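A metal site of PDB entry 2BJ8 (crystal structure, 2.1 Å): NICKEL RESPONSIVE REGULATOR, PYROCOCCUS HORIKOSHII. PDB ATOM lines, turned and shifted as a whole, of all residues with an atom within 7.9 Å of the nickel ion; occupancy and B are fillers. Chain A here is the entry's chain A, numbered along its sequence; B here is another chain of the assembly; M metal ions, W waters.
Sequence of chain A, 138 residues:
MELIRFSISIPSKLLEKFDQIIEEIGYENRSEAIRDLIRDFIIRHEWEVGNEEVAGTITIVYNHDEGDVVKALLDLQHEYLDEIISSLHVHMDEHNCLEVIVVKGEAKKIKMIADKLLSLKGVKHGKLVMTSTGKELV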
ATOM      1  N   ASN A  63     -20.574  22.920 -12.367  1.00  0.00           N
ATOM      2  CA  ASN A  63     -21.671  22.046 -12.743  1.00  0.00           C
ATOM      3  C   ASN A  63     -21.001  21.140 -13.767  1.00  0.00           C
ATOM      4  O   ASN A  63     -20.594  21.605 -14.837  1.00  0.00           O
ATOM      5  CB  ASN A  63     -22.769  22.845 -13.428  1.00  0.00           C
ATOM      6  CG  ASN A  63     -23.952  21.985 -13.805  1.00  0.00           C
ATOM      7  OD1 ASN A  63     -23.791  20.908 -14.387  1.00  0.00           O
ATOM      8  ND2 ASN A  63     -25.142  22.464 -13.482  1.00  0.00           N
ATOM      9  N   HIS A  64     -20.868  19.861 -13.456  1.00  0.00           N
ATOM     10  CA  HIS A  64     -20.191  18.962 -14.372  1.00  0.00           C
ATOM     11  C   HIS A  64     -20.951  18.743 -15.680  1.00  0.00           C
ATOM     12  O   HIS A  64     -20.400  18.168 -16.617  1.00  0.00           O
ATOM     13  CB  HIS A  64     -19.893  17.615 -13.709  1.00  0.00           C
ATOM     14  CG  HIS A  64     -21.123  16.809 -13.432  1.00  0.00           C
ATOM     15  ND1 HIS A  64     -21.826  16.910 -12.255  1.00  0.00           N
ATOM     16  CD2 HIS A  64     -21.780  15.894 -14.181  1.00  0.00           C
ATOM     17  CE1 HIS A  64     -22.868  16.089 -12.284  1.00  0.00           C
ATOM     18  NE2 HIS A  64     -22.852  15.458 -13.448  1.00  0.00           N
ATOM     19  N   ASP A  65     -22.189  19.197 -15.739  1.00  0.00           N
ATOM     20  CA  ASP A  65     -22.986  19.035 -16.948  1.00  0.00           C
ATOM     21  C   ASP A  65     -22.922  20.257 -17.863  1.00  0.00           C
ATOM     22  O   ASP A  65     -23.433  20.210 -18.985  1.00  0.00           O
ATOM     23  CB  ASP A  65     -24.439  18.732 -16.597  1.00  0.00           C
ATOM     24  CG  ASP A  65     -24.604  17.382 -15.936  1.00  0.00           C
ATOM     25  OD1 ASP A  65     -24.044  16.401 -16.464  1.00  0.00           O
ATOM     26  OD2 ASP A  65     -25.284  17.309 -14.881  1.00  0.00           O
ATOM     27  N   GLU A  66     -22.284  21.320 -17.397  1.00  0.00           N
ATOM     28  CA  GLU A  66     -22.164  22.547 -18.190  1.00  0.00           C
ATOM     29  C   GLU A  66     -21.040  22.438 -19.217  1.00  0.00           C
ATOM     30  O   GLU A  66     -19.959  21.920 -18.930  1.00  0.00           O
ATOM     31  CB  GLU A  66     -21.910  23.738 -17.279  1.00  0.00           C
ATOM     32  CG  GLU A  66     -22.002  25.087 -17.975  1.00  0.00           C
ATOM     33  CD  GLU A  66     -21.779  26.250 -17.029  1.00  0.00           C
ATOM     34  OE1 GLU A  66     -22.438  26.294 -15.966  1.00  0.00           O
ATOM     35  OE2 GLU A  66     -20.947  27.122 -17.349  1.00  0.00           O
ATOM     36  N   ASP A  93     -24.376  17.976  -5.232  1.00  0.00           N
ATOM     37  CA  ASP A  93     -25.756  17.650  -5.546  1.00  0.00           C
ATOM     38  C   ASP A  93     -25.752  17.046  -6.920  1.00  0.00           C
ATOM     39  O   ASP A  93     -24.687  16.782  -7.490  1.00  0.00           O
ATOM     40  CB  ASP A  93     -26.648  18.921  -5.522  1.00  0.00           C
ATOM     41  CG  ASP A  93     -26.232  19.963  -6.552  1.00  0.00           C
ATOM     42  OD1 ASP A  93     -25.901  19.589  -7.703  1.00  0.00           O
ATOM     43  OD2 ASP A  93     -26.252  21.164  -6.212  1.00  0.00           O
ATOM     44  N   GLU A  94     -26.937  16.850  -7.466  1.00  0.00           N
ATOM     45  CA  GLU A  94     -27.081  16.249  -8.776  1.00  0.00           C
ATOM     46  C   GLU A  94     -26.170  16.817  -9.851  1.00  0.00           C
ATOM     47  O   GLU A  94     -25.671  16.071 -10.695  1.00  0.00           O
ATOM     48  CB  GLU A  94     -28.537  16.383  -9.226  1.00  0.00           C
ATOM     49  CG  GLU A  94     -28.827  15.766 -10.570  1.00  0.00           C
ATOM     50  CD  GLU A  94     -30.263  15.972 -11.006  1.00  0.00           C
ATOM     51  OE1 GLU A  94     -30.622  15.503 -12.107  1.00  0.00           O
ATOM     52  OE2 GLU A  94     -31.032  16.588 -10.239  1.00  0.00           O
ATOM     53  N   HIS A  95     -25.923  18.123  -9.823  1.00  0.00           N
ATOM     54  CA  HIS A  95     -25.107  18.771 -10.848  1.00  0.00           C
ATOM     55  C   HIS A  95     -23.782  19.381 -10.413  1.00  0.00           C
ATOM     56  O   HIS A  95     -22.823  19.408 -11.186  1.00  0.00           O
ATOM     57  CB  HIS A  95     -25.909  19.881 -11.529  1.00  0.00           C
ATOM     58  CG  HIS A  95     -27.209  19.426 -12.131  1.00  0.00           C
ATOM     59  ND1 HIS A  95     -27.274  18.640 -13.264  1.00  0.00           N
ATOM     60  CD2 HIS A  95     -28.489  19.638 -11.745  1.00  0.00           C
ATOM     61  CE1 HIS A  95     -28.544  18.391 -13.549  1.00  0.00           C
ATOM     62  NE2 HIS A  95     -29.301  18.991 -12.644  1.00  0.00           N
ATOM     63  N   ASN A  96     -23.721  19.875  -9.190  1.00  0.00           N
ATOM     64  CA  ASN A  96     -22.523  20.553  -8.711  1.00  0.00           C
ATOM     65  C   ASN A  96     -21.439  19.715  -8.041  1.00  0.00           C
ATOM     66  O   ASN A  96     -21.715  18.830  -7.240  1.00  0.00           O
ATOM     67  CB  ASN A  96     -22.945  21.697  -7.809  1.00  0.00           C
ATOM     68  CG  ASN A  96     -23.774  22.724  -8.552  1.00  0.00           C
ATOM     69  OD1 ASN A  96     -23.274  23.430  -9.413  1.00  0.00           O
ATOM     70  ND2 ASN A  96     -25.054  22.796  -8.222  1.00  0.00           N
ATOM     71  N   CYS A  97     -20.203  20.028  -8.393  1.00  0.00           N
ATOM     72  CA  CYS A  97     -19.037  19.344  -7.845  1.00  0.00           C
ATOM     73  C   CYS A  97     -18.061  20.349  -7.256  1.00  0.00           C
ATOM     74  O   CYS A  97     -17.903  21.457  -7.761  1.00  0.00           O
ATOM     75  CB  CYS A  97     -18.297  18.568  -8.934  1.00  0.00           C
ATOM     76  SG  CYS A  97     -19.239  17.321  -9.833  1.00  0.00           S
ATOM     77  N   LYS B  71     -17.767  11.223 -18.368  1.00  0.00           N
ATOM     78  CA  LYS B  71     -19.123  11.704 -18.155  1.00  0.00           C
ATOM     79  C   LYS B  71     -19.962  10.619 -17.508  1.00  0.00           C
ATOM     80  O   LYS B  71     -20.772  10.883 -16.614  1.00  0.00           O
ATOM     81  CB  LYS B  71     -19.730  12.118 -19.496  1.00  0.00           C
ATOM     82  CG  LYS B  71     -21.078  12.805 -19.392  1.00  0.00           C
ATOM     83  CD  LYS B  71     -21.572  13.263 -20.763  1.00  0.00           C
ATOM     84  CE  LYS B  71     -22.866  14.068 -20.666  1.00  0.00           C
ATOM     85  NZ  LYS B  71     -23.991  13.265 -20.116  1.00  0.00           N
ATOM     86  N   ALA B  72     -19.793   9.383 -17.972  1.00  0.00           N
ATOM     87  CA  ALA B  72     -20.534   8.253 -17.443  1.00  0.00           C
ATOM     88  C   ALA B  72     -20.234   8.081 -15.948  1.00  0.00           C
ATOM     89  O   ALA B  72     -21.155   7.842 -15.154  1.00  0.00           O
ATOM     90  CB  ALA B  72     -20.163   6.983 -18.212  1.00  0.00           C
ATOM     91  N   LEU B  74     -19.150  10.364 -13.703  1.00  0.00           N
ATOM     92  CA  LEU B  74     -19.759  11.445 -12.937  1.00  0.00           C
ATOM     93  C   LEU B  74     -21.258  11.240 -12.759  1.00  0.00           C
ATOM     94  O   LEU B  74     -21.774  11.363 -11.637  1.00  0.00           O
ATOM     95  CB  LEU B  74     -19.492  12.783 -13.627  1.00  0.00           C
ATOM     96  CG  LEU B  74     -18.098  13.374 -13.444  1.00  0.00           C
ATOM     97  CD1 LEU B  74     -17.921  14.568 -14.365  1.00  0.00           C
ATOM     98  CD2 LEU B  74     -17.897  13.763 -11.983  1.00  0.00           C
ATOM     99  N   ASP B  75     -21.949  10.925 -13.848  1.00  0.00           N
ATOM    100  CA  ASP B  75     -23.389  10.728 -13.790  1.00  0.00           C
ATOM    101  C   ASP B  75     -23.771   9.610 -12.828  1.00  0.00           C
ATOM    102  O   ASP B  75     -24.695   9.754 -12.026  1.00  0.00           O
ATOM    103  CB  ASP B  75     -23.943  10.432 -15.185  1.00  0.00           C
ATOM    104  CG  ASP B  75     -23.975  11.678 -16.067  1.00  0.00           C
ATOM    105  OD1 ASP B  75     -24.320  11.541 -17.265  1.00  0.00           O
ATOM    106  OD2 ASP B  75     -23.671  12.783 -15.571  1.00  0.00           O
ATOM    107  N   LEU B  76     -23.044   8.500 -12.892  1.00  0.00           N
ATOM    108  CA  LEU B  76     -23.323   7.385 -11.999  1.00  0.00           C
ATOM    109  C   LEU B  76     -23.125   7.812 -10.539  1.00  0.00           C
ATOM    110  O   LEU B  76     -23.991   7.609  -9.701  1.00  0.00           O
ATOM    111  CB  LEU B  76     -22.393   6.199 -12.310  1.00  0.00           C
ATOM    112  CG  LEU B  76     -22.806   5.314 -13.485  1.00  0.00           C
ATOM    113  CD1 LEU B  76     -21.764   4.230 -13.719  1.00  0.00           C
ATOM    114  CD2 LEU B  76     -24.161   4.683 -13.167  1.00  0.00           C
ATOM    115  N   HIS B  78     -23.030  10.867  -9.144  1.00  0.00           N
ATOM    116  CA  HIS B  78     -23.955  11.881  -8.650  1.00  0.00           C
ATOM    117  C   HIS B  78     -25.334  11.309  -8.377  1.00  0.00           C
ATOM    118  O   HIS B  78     -26.193  11.961  -7.777  1.00  0.00           O
ATOM    119  CB  HIS B  78     -24.026  13.046  -9.648  1.00  0.00           C
ATOM    120  CG  HIS B  78     -22.936  14.051  -9.463  1.00  0.00           C
ATOM    121  ND1 HIS B  78     -23.138  15.260  -8.827  1.00  0.00           N
ATOM    122  CD2 HIS B  78     -21.622  14.011  -9.773  1.00  0.00           C
ATOM    123  CE1 HIS B  78     -22.005  15.917  -8.758  1.00  0.00           C
ATOM    124  NE2 HIS B  78     -21.055  15.182  -9.324  1.00  0.00           N
HETATM  125 NI    NI M   1     -24.447  14.834 -15.064  1.00  0.00          NI
HETATM  126  O   HOH W   1     -25.583  14.741 -13.173  1.00  0.00           O
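Water W1 lies within hydrogen-bond range of the backbone carbonyl oxygen (O) of Glu 94 (2.8 Å) and the side-chain carboxylate (OD2) of Asp 65 (3.1 Å).
OD1 of Asp 65 binds the nickel ion (2.1 Å). Water W1 binds the nickel ion (2.2 Å). OD2 of Asp 75 of chain B binds the nickel ion, 2.3 Å away. A ring nitrogen (NE2) of His 64 binds the nickel ion. Slightly farther from the nickel ion lies OD2 of Asp 65 (2.6 Å).
The side-chain carboxylate (OD2) of Asp 65 sits at hydrogen-bond distance from a ring nitrogen (ND1) of His 95, 2.9 Å away. N of Asp 65 sits at hydrogen-bond distance from OD1 of Asn 63, at 2.7 Å. The side-chain carboxylate of Asp 75 of chain B lies within salt-bridge range of the side-chain amino group of Lys 71 of chain B, at 3.3 Å. A ring nitrogen (ND1) of His 64 sits at hydrogen-bond distance from the backbone carbonyl oxygen (O) of His 95, 2.9 Å away. ND1 of His 64 lies close to NE2 of His 78 of chain B, 3.5 Å away. A ring nitrogen (ND1) of His 64 lies close to the side-chain sulfur (SG) of Cys 97, at 3.6 Å.
Three residues have an atom within 4 Å of the nickel ion: His 64, Asp 65 and Asp 75 of chain B. The nearest printed residue that does not touch the nickel ion is Glu 94 (4.7 Å).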
